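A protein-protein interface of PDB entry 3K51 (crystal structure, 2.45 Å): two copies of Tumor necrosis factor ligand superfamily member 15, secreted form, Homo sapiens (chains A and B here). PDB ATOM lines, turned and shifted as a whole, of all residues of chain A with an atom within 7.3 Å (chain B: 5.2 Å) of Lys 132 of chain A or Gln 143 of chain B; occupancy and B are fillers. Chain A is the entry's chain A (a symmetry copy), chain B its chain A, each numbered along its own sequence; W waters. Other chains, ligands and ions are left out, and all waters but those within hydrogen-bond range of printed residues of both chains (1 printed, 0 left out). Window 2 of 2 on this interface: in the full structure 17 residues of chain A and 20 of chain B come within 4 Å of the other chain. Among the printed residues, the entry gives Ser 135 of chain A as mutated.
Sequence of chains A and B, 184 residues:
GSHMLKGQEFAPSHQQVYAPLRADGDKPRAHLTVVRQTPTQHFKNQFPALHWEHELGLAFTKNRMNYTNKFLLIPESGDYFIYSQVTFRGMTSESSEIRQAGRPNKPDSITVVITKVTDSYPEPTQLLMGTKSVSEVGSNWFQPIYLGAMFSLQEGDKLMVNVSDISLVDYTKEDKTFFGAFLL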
ATOM      1  N   PRO A 107     -11.954  12.798  37.511  1.00  0.00           N
ATOM      2  CA  PRO A 107     -12.600  12.526  36.225  1.00  0.00           C
ATOM      3  C   PRO A 107     -11.691  12.869  35.046  1.00  0.00           C
ATOM      4  O   PRO A 107     -10.480  13.026  35.221  1.00  0.00           O
ATOM      5  CB  PRO A 107     -13.821  13.455  36.245  1.00  0.00           C
ATOM      6  CG  PRO A 107     -13.452  14.548  37.185  1.00  0.00           C
ATOM      7  CD  PRO A 107     -12.591  13.914  38.231  1.00  0.00           C
ATOM      8  N   ASP A 108     -12.274  12.975  33.856  1.00  0.00           N
ATOM      9  CA  ASP A 108     -11.510  13.275  32.648  1.00  0.00           C
ATOM     10  C   ASP A 108     -11.354  14.774  32.435  1.00  0.00           C
ATOM     11  O   ASP A 108     -10.422  15.220  31.768  1.00  0.00           O
ATOM     12  CB  ASP A 108     -12.165  12.639  31.423  1.00  0.00           C
ATOM     13  CG  ASP A 108     -11.462  11.373  30.976  1.00  0.00           C
ATOM     14  OD1 ASP A 108     -10.264  11.211  31.293  1.00  0.00           O
ATOM     15  OD2 ASP A 108     -12.105  10.544  30.299  1.00  0.00           O
ATOM     16  N   SER A 109     -12.274  15.549  32.999  1.00  0.00           N
ATOM     17  CA  SER A 109     -12.256  16.989  32.824  1.00  0.00           C
ATOM     18  C   SER A 109     -12.931  17.721  33.976  1.00  0.00           C
ATOM     19  O   SER A 109     -13.808  17.175  34.649  1.00  0.00           O
ATOM     20  CB  SER A 109     -12.915  17.375  31.495  1.00  0.00           C
ATOM     21  OG  SER A 109     -14.300  17.078  31.506  1.00  0.00           O
ATOM     22  N   ILE A 110     -12.501  18.957  34.210  1.00  0.00           N
ATOM     23  CA  ILE A 110     -13.207  19.865  35.100  1.00  0.00           C
ATOM     24  C   ILE A 110     -13.763  21.039  34.293  1.00  0.00           C
ATOM     25  O   ILE A 110     -13.139  21.494  33.336  1.00  0.00           O
ATOM     26  CB  ILE A 110     -12.289  20.386  36.227  1.00  0.00           C
ATOM     27  CG1 ILE A 110     -10.999  20.968  35.645  1.00  0.00           C
ATOM     28  CG2 ILE A 110     -11.965  19.266  37.210  1.00  0.00           C
ATOM     29  CD1 ILE A 110      -9.989  21.395  36.693  1.00  0.00           C
ATOM     30  N   THR A 111     -14.947  21.509  34.668  1.00  0.00           N
ATOM     31  CA  THR A 111     -15.645  22.518  33.885  1.00  0.00           C
ATOM     32  C   THR A 111     -16.355  23.535  34.759  1.00  0.00           C
ATOM     33  O   THR A 111     -17.048  23.171  35.711  1.00  0.00           O
ATOM     34  CB  THR A 111     -16.669  21.875  32.925  1.00  0.00           C
ATOM     35  OG1 THR A 111     -15.974  21.151  31.899  1.00  0.00           O
ATOM     36  CG2 THR A 111     -17.549  22.940  32.279  1.00  0.00           C
ATOM     37  N   VAL A 112     -16.156  24.816  34.441  1.00  0.00           N
ATOM     38  CA  VAL A 112     -16.944  25.903  35.022  1.00  0.00           C
ATOM     39  C   VAL A 112     -17.758  26.580  33.922  1.00  0.00           C
ATOM     40  O   VAL A 112     -17.224  26.906  32.863  1.00  0.00           O
ATOM     41  CB  VAL A 112     -16.044  26.967  35.676  1.00  0.00           C
ATOM     42  CG1 VAL A 112     -16.892  28.045  36.347  1.00  0.00           C
ATOM     43  CG2 VAL A 112     -15.107  26.330  36.669  1.00  0.00           C
ATOM     44  N   GLY A 130     -15.264  27.619  30.953  1.00  0.00           N
ATOM     45  CA  GLY A 130     -13.872  27.228  31.103  1.00  0.00           C
ATOM     46  C   GLY A 130     -13.765  25.739  31.343  1.00  0.00           C
ATOM     47  O   GLY A 130     -14.207  25.236  32.378  1.00  0.00           O
ATOM     48  N   THR A 131     -13.201  25.020  30.381  1.00  0.00           N
ATOM     49  CA  THR A 131     -13.158  23.559  30.464  1.00  0.00           C
ATOM     50  C   THR A 131     -11.751  23.004  30.234  1.00  0.00           C
ATOM     51  O   THR A 131     -11.069  23.380  29.277  1.00  0.00           O
ATOM     52  CB  THR A 131     -14.179  22.905  29.500  1.00  0.00           C
ATOM     53  OG1 THR A 131     -14.320  21.517  29.819  1.00  0.00           O
ATOM     54  CG2 THR A 131     -13.740  23.054  28.052  1.00  0.00           C
ATOM     55  N   LYS A 132     -11.326  22.106  31.115  1.00  0.00           N
ATOM     56  CA  LYS A 132      -9.954  21.615  31.100  1.00  0.00           C
ATOM     57  C   LYS A 132      -9.893  20.105  31.329  1.00  0.00           C
ATOM     58  O   LYS A 132     -10.590  19.566  32.189  1.00  0.00           O
ATOM     59  CB  LYS A 132      -9.117  22.342  32.156  1.00  0.00           C
ATOM     60  CG  LYS A 132      -7.619  22.188  31.980  1.00  0.00           C
ATOM     61  CD  LYS A 132      -6.856  23.027  32.999  1.00  0.00           C
ATOM     62  CE  LYS A 132      -5.393  23.188  32.604  1.00  0.00           C
ATOM     63  NZ  LYS A 132      -4.707  21.873  32.471  1.00  0.00           N
ATOM     64  N   SER A 133      -9.059  19.424  30.547  1.00  0.00           N
ATOM     65  CA  SER A 133      -8.883  17.979  30.692  1.00  0.00           C
ATOM     66  C   SER A 133      -7.884  17.666  31.799  1.00  0.00           C
ATOM     67  O   SER A 133      -6.856  18.329  31.922  1.00  0.00           O
ATOM     68  CB  SER A 133      -8.431  17.345  29.369  1.00  0.00           C
ATOM     69  OG  SER A 133      -7.119  17.754  29.024  1.00  0.00           O
ATOM     70  N   VAL A 134      -8.202  16.663  32.615  1.00  0.00           N
ATOM     71  CA  VAL A 134      -7.362  16.299  33.755  1.00  0.00           C
ATOM     72  C   VAL A 134      -6.592  15.011  33.473  1.00  0.00           C
ATOM     73  O   VAL A 134      -7.187  13.983  33.143  1.00  0.00           O
ATOM     74  CB  VAL A 134      -8.198  16.116  35.039  1.00  0.00           C
ATOM     75  CG1 VAL A 134      -7.293  15.895  36.233  1.00  0.00           C
ATOM     76  CG2 VAL A 134      -9.090  17.320  35.263  1.00  0.00           C
ATOM     77  N   SER A 135      -5.269  15.072  33.607  1.00  0.00           N
ATOM     78  CA  SER A 135      -4.409  13.933  33.278  1.00  0.00           C
ATOM     79  C   SER A 135      -4.199  13.014  34.481  1.00  0.00           C
ATOM     80  O   SER A 135      -3.286  13.221  35.284  1.00  0.00           O
ATOM     81  CB  SER A 135      -3.060  14.418  32.741  1.00  0.00           C
ATOM     82  OG  SER A 135      -2.418  13.406  31.985  1.00  0.00           O
ATOM     83  N   GLN A 143      -6.225  23.045  40.806  1.00  0.00           N
ATOM     84  CA  GLN A 143      -6.215  23.857  39.598  1.00  0.00           C
ATOM     85  C   GLN A 143      -7.342  24.872  39.625  1.00  0.00           C
ATOM     86  O   GLN A 143      -8.483  24.522  39.916  1.00  0.00           O
ATOM     87  CB  GLN A 143      -6.385  22.967  38.372  1.00  0.00           C
ATOM     88  CG  GLN A 143      -5.177  22.875  37.504  1.00  0.00           C
ATOM     89  CD  GLN A 143      -5.462  22.145  36.219  1.00  0.00           C
ATOM     90  OE1 GLN A 143      -4.678  22.199  35.272  1.00  0.00           O
ATOM     91  NE2 GLN A 143      -6.592  21.450  36.174  1.00  0.00           N
ATOM     92  N   PRO A 144      -7.028  26.135  39.297  1.00  0.00           N
ATOM     93  CA  PRO A 144      -8.041  27.166  39.186  1.00  0.00           C
ATOM     94  C   PRO A 144      -8.536  27.329  37.754  1.00  0.00           C
ATOM     95  O   PRO A 144      -7.790  27.104  36.807  1.00  0.00           O
ATOM     96  CB  PRO A 144      -7.299  28.418  39.624  1.00  0.00           C
ATOM     97  CG  PRO A 144      -5.886  28.183  39.182  1.00  0.00           C
ATOM     98  CD  PRO A 144      -5.666  26.683  39.178  1.00  0.00           C
ATOM     99  N   ILE A 145      -9.793  27.713  37.606  1.00  0.00           N
ATOM    100  CA  ILE A 145     -10.310  28.117  36.323  1.00  0.00           C
ATOM    101  C   ILE A 145     -10.913  29.512  36.436  1.00  0.00           C
ATOM    102  O   ILE A 145     -11.822  29.737  37.236  1.00  0.00           O
ATOM    103  CB  ILE A 145     -11.352  27.102  35.786  1.00  0.00           C
ATOM    104  CG1 ILE A 145     -10.654  25.796  35.381  1.00  0.00           C
ATOM    105  CG2 ILE A 145     -12.114  27.680  34.604  1.00  0.00           C
ATOM    106  CD1 ILE A 145     -11.598  24.715  34.865  1.00  0.00           C
ATOM    107  N   SER A 164     -18.752  21.045  36.967  1.00  0.00           N
ATOM    108  CA  SER A 164     -18.906  19.651  36.572  1.00  0.00           C
ATOM    109  C   SER A 164     -19.073  18.719  37.784  1.00  0.00           C
ATOM    110  O   SER A 164     -19.932  17.838  37.785  1.00  0.00           O
ATOM    111  CB  SER A 164     -17.714  19.209  35.722  1.00  0.00           C
ATOM    112  OG  SER A 164     -16.499  19.704  36.256  1.00  0.00           O
ATOM    113  N   VAL B  86      -9.080  31.735  24.576  1.00  0.00           N
ATOM    114  CA  VAL B  86      -9.046  30.759  23.510  1.00  0.00           C
ATOM    115  C   VAL B  86      -8.944  29.370  24.112  1.00  0.00           C
ATOM    116  O   VAL B  86      -7.999  29.068  24.837  1.00  0.00           O
ATOM    117  CB  VAL B  86      -7.852  30.991  22.564  1.00  0.00           C
ATOM    118  CG1 VAL B  86      -7.797  29.896  21.491  1.00  0.00           C
ATOM    119  CG2 VAL B  86      -7.938  32.380  21.924  1.00  0.00           C
ATOM    120  N   THR B  87      -9.943  28.536  23.848  1.00  0.00           N
ATOM    121  CA  THR B  87      -9.875  27.146  24.266  1.00  0.00           C
ATOM    122  C   THR B  87      -9.155  26.322  23.208  1.00  0.00           C
ATOM    123  O   THR B  87      -9.529  26.329  22.028  1.00  0.00           O
ATOM    124  CB  THR B  87     -11.274  26.552  24.547  1.00  0.00           C
ATOM    125  OG1 THR B  87     -11.900  27.283  25.612  1.00  0.00           O
ATOM    126  CG2 THR B  87     -11.158  25.093  24.954  1.00  0.00           C
ATOM    127  N   PHE B  88      -8.092  25.651  23.624  1.00  0.00           N
ATOM    128  CA  PHE B  88      -7.331  24.800  22.727  1.00  0.00           C
ATOM    129  C   PHE B  88      -7.710  23.343  22.925  1.00  0.00           C
ATOM    130  O   PHE B  88      -7.938  22.902  24.050  1.00  0.00           O
ATOM    131  CB  PHE B  88      -5.835  24.988  22.962  1.00  0.00           C
ATOM    132  CG  PHE B  88      -5.327  26.339  22.568  1.00  0.00           C
ATOM    133  CD1 PHE B  88      -4.853  26.570  21.285  1.00  0.00           C
ATOM    134  CD2 PHE B  88      -5.319  27.382  23.477  1.00  0.00           C
ATOM    135  CE1 PHE B  88      -4.381  27.816  20.919  1.00  0.00           C
ATOM    136  CE2 PHE B  88      -4.846  28.630  23.117  1.00  0.00           C
ATOM    137  CZ  PHE B  88      -4.376  28.847  21.837  1.00  0.00           C
ATOM    138  N   ARG B  89      -7.782  22.600  21.827  1.00  0.00           N
ATOM    139  CA  ARG B  89      -8.082  21.174  21.887  1.00  0.00           C
ATOM    140  C   ARG B  89      -7.189  20.382  20.942  1.00  0.00           C
ATOM    141  O   ARG B  89      -6.970  20.776  19.794  1.00  0.00           O
ATOM    142  CB  ARG B  89      -9.561  20.910  21.572  1.00  0.00           C
ATOM    143  CG  ARG B  89     -10.019  21.444  20.223  1.00  0.00           C
ATOM    144  CD  ARG B  89     -11.333  20.814  19.796  1.00  0.00           C
ATOM    145  NE  ARG B  89     -11.794  21.334  18.512  1.00  0.00           N
ATOM    146  CZ  ARG B  89     -11.102  21.251  17.380  1.00  0.00           C
ATOM    147  NH1 ARG B  89     -11.600  21.747  16.258  1.00  0.00           N
ATOM    148  NH2 ARG B  89      -9.905  20.679  17.374  1.00  0.00           N
ATOM    149  N   ILE B 110       1.127  25.903  23.510  1.00  0.00           N
ATOM    150  CA  ILE B 110       0.061  26.692  22.911  1.00  0.00           C
ATOM    151  C   ILE B 110       0.174  28.142  23.383  1.00  0.00           C
ATOM    152  O   ILE B 110       0.551  28.402  24.525  1.00  0.00           O
ATOM    153  CB  ILE B 110      -1.333  26.127  23.264  1.00  0.00           C
ATOM    154  CG1 ILE B 110      -1.472  25.946  24.777  1.00  0.00           C
ATOM    155  CG2 ILE B 110      -1.566  24.801  22.551  1.00  0.00           C
ATOM    156  CD1 ILE B 110      -2.770  25.285  25.200  1.00  0.00           C
ATOM    157  N   LYS B 132       1.593  28.465  27.264  1.00  0.00           N
ATOM    158  CA  LYS B 132       1.580  27.275  28.107  1.00  0.00           C
ATOM    159  C   LYS B 132       2.225  26.080  27.406  1.00  0.00           C
ATOM    160  O   LYS B 132       1.989  25.837  26.223  1.00  0.00           O
ATOM    161  CB  LYS B 132       0.146  26.932  28.521  1.00  0.00           C
ATOM    162  CG  LYS B 132       0.047  25.961  29.681  1.00  0.00           C
ATOM    163  CD  LYS B 132      -1.403  25.756  30.103  1.00  0.00           C
ATOM    164  CE  LYS B 132      -1.496  25.104  31.478  1.00  0.00           C
ATOM    165  NZ  LYS B 132      -0.806  23.785  31.513  1.00  0.00           N
ATOM    166  N   VAL B 134       2.745  22.149  26.605  1.00  0.00           N
ATOM    167  CA  VAL B 134       1.852  20.995  26.522  1.00  0.00           C
ATOM    168  C   VAL B 134       2.628  19.694  26.706  1.00  0.00           C
ATOM    169  O   VAL B 134       3.596  19.432  25.988  1.00  0.00           O
ATOM    170  CB  VAL B 134       1.108  20.952  25.171  1.00  0.00           C
ATOM    171  CG1 VAL B 134       0.077  19.842  25.169  1.00  0.00           C
ATOM    172  CG2 VAL B 134       0.451  22.287  24.887  1.00  0.00           C
ATOM    173  N   TRP B 141      -6.715  16.061  24.711  1.00  0.00           N
ATOM    174  CA  TRP B 141      -6.700  17.119  25.713  1.00  0.00           C
ATOM    175  C   TRP B 141      -7.392  18.394  25.222  1.00  0.00           C
ATOM    176  O   TRP B 141      -7.535  18.617  24.018  1.00  0.00           O
ATOM    177  CB  TRP B 141      -5.260  17.433  26.133  1.00  0.00           C
ATOM    178  CG  TRP B 141      -4.393  17.867  24.986  1.00  0.00           C
ATOM    179  CD1 TRP B 141      -3.613  17.070  24.199  1.00  0.00           C
ATOM    180  CD2 TRP B 141      -4.237  19.203  24.483  1.00  0.00           C
ATOM    181  NE1 TRP B 141      -2.974  17.824  23.244  1.00  0.00           N
ATOM    182  CE2 TRP B 141      -3.342  19.137  23.394  1.00  0.00           C
ATOM    183  CE3 TRP B 141      -4.766  20.446  24.848  1.00  0.00           C
ATOM    184  CZ2 TRP B 141      -2.962  20.266  22.669  1.00  0.00           C
ATOM    185  CZ3 TRP B 141      -4.392  21.564  24.125  1.00  0.00           C
ATOM    186  CH2 TRP B 141      -3.497  21.466  23.047  1.00  0.00           C
ATOM    187  N   PHE B 142      -7.829  19.216  26.170  1.00  0.00           N
ATOM    188  CA  PHE B 142      -8.283  20.570  25.870  1.00  0.00           C
ATOM    189  C   PHE B 142      -7.982  21.518  27.025  1.00  0.00           C
ATOM    190  O   PHE B 142      -7.899  21.102  28.185  1.00  0.00           O
ATOM    191  CB  PHE B 142      -9.776  20.596  25.512  1.00  0.00           C
ATOM    192  CG  PHE B 142     -10.634  19.756  26.412  1.00  0.00           C
ATOM    193  CD1 PHE B 142     -10.846  18.410  26.134  1.00  0.00           C
ATOM    194  CD2 PHE B 142     -11.250  20.311  27.522  1.00  0.00           C
ATOM    195  CE1 PHE B 142     -11.642  17.633  26.958  1.00  0.00           C
ATOM    196  CE2 PHE B 142     -12.049  19.539  28.347  1.00  0.00           C
ATOM    197  CZ  PHE B 142     -12.244  18.195  28.064  1.00  0.00           C
ATOM    198  N   GLN B 143      -7.806  22.792  26.698  1.00  0.00           N
ATOM    199  CA  GLN B 143      -7.292  23.769  27.649  1.00  0.00           C
ATOM    200  C   GLN B 143      -7.634  25.178  27.206  1.00  0.00           C
ATOM    201  O   GLN B 143      -7.423  25.531  26.048  1.00  0.00           O
ATOM    202  CB  GLN B 143      -5.777  23.641  27.757  1.00  0.00           C
ATOM    203  CG  GLN B 143      -5.294  23.123  29.068  1.00  0.00           C
ATOM    204  CD  GLN B 143      -3.795  23.201  29.186  1.00  0.00           C
ATOM    205  OE1 GLN B 143      -3.238  23.072  30.276  1.00  0.00           O
ATOM    206  NE2 GLN B 143      -3.126  23.411  28.060  1.00  0.00           N
ATOM    207  N   PRO B 144      -8.144  26.000  28.136  1.00  0.00           N
ATOM    208  CA  PRO B 144      -8.409  27.397  27.856  1.00  0.00           C
ATOM    209  C   PRO B 144      -7.245  28.292  28.262  1.00  0.00           C
ATOM    210  O   PRO B 144      -6.524  27.987  29.206  1.00  0.00           O
ATOM    211  CB  PRO B 144      -9.620  27.693  28.725  1.00  0.00           C
ATOM    212  CG  PRO B 144      -9.443  26.804  29.920  1.00  0.00           C
ATOM    213  CD  PRO B 144      -8.651  25.596  29.459  1.00  0.00           C
ATOM    214  N   ILE B 145      -7.067  29.388  27.543  1.00  0.00           N
ATOM    215  CA  ILE B 145      -6.151  30.420  27.959  1.00  0.00           C
ATOM    216  C   ILE B 145      -6.888  31.753  28.030  1.00  0.00           C
ATOM    217  O   ILE B 145      -7.456  32.207  27.037  1.00  0.00           O
ATOM    218  CB  ILE B 145      -4.929  30.511  27.010  1.00  0.00           C
ATOM    219  CG1 ILE B 145      -4.028  29.281  27.195  1.00  0.00           C
ATOM    220  CG2 ILE B 145      -4.137  31.784  27.265  1.00  0.00           C
ATOM    221  CD1 ILE B 145      -2.806  29.257  26.283  1.00  0.00           C
HETATM  222  O   HOH W   1     -13.107  26.271  27.886  1.00  0.00           O
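Of the 16 printed residues of chain A, 4 touch a printed residue of chain B. Hydrophobic or aromatic side chains of chain B within 4 Å of the printed part of chain A: Trp 141, Phe 142 and Pro 144. Among the printed residues, 7 pairs touch across the chains. Among the printed residues, no Asp or Glu carboxylate lies within 4 Å of a Lys or Arg side-chain nitrogen of the other chain.
The backbone NH (N) of Phe 88 of chain B is in hydrogen-bond range of the backbone carbonyl oxygen (O) of Gln 143 of chain B (2.5 Å). NZ of Lys 132 of chain B sits at hydrogen-bond distance from OE1 of Gln 143 of chain B (2.8 Å). The backbone NH (N) of Ile 110 of chain A is in hydrogen-bond range of the backbone carbonyl oxygen (O) of Lys 132 of chain A. OG1 of Thr 131 of chain A is in hydrogen-bond range of OG1 of Thr 111 of chain A (2.7 Å). OE1 of Gln 143 of chain A is in hydrogen-bond range of NZ of Lys 132 of chain A (2.8 Å).
Of chain B, only Phe 142 (3.6 Å) and Gln 143 (2.9 Å) come within 4 Å of Lys 132 of chain A. Of chain A, only Lys 132 comes within 4 Å of Gln 143 of chain B. Printed residues of chain A within 4 Å of Pro 144 of chain B: Thr 131 (3.3 Å). Of the printed residues of chain B, Thr 131 of chain A touches Phe 142 and Pro 144. The nearest residue of chain A that does not touch Gln 143 of chain B is Thr 131 of chain A (4.1 Å).
The backbone NH of Ser 133 of chain A lies within hydrogen-bond range of the backbone carbonyl oxygen of Phe 142 of chain B, 3.1 Å away. OE1 of Gln 143 of chain B lies within hydrogen-bond range of NZ of Lys 132 of chain A (2.9 Å).
Lys 132 of chain A touches Gln 143 of chain B, but with the chains exchanged Gln 143 of chain A does not touch Lys 132 of chain B (5.6 Å). Of the 7 pairs that touch across the chains among the printed residues, none has its exchanged pair printed and touching as well.
Water W1 bridges OG1 of Thr 87 of chain B (2.8 Å) and N of Thr 131 of chain A (2.8 Å).
Among the printed residues, merely in contact across the chains: Ser 109 of chain A with Phe 142 of chain B (3.6 Å), Thr 131 of chain A with Phe 142 of chain B (3.4 Å), Thr 131 of chain A with Pro 144 of chain B (3.3 Å), Lys 132 of chain A with Phe 142 of chain B (3.6 Å) and Ser 133 of chain A with Trp 141 of chain B (3.4 Å).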
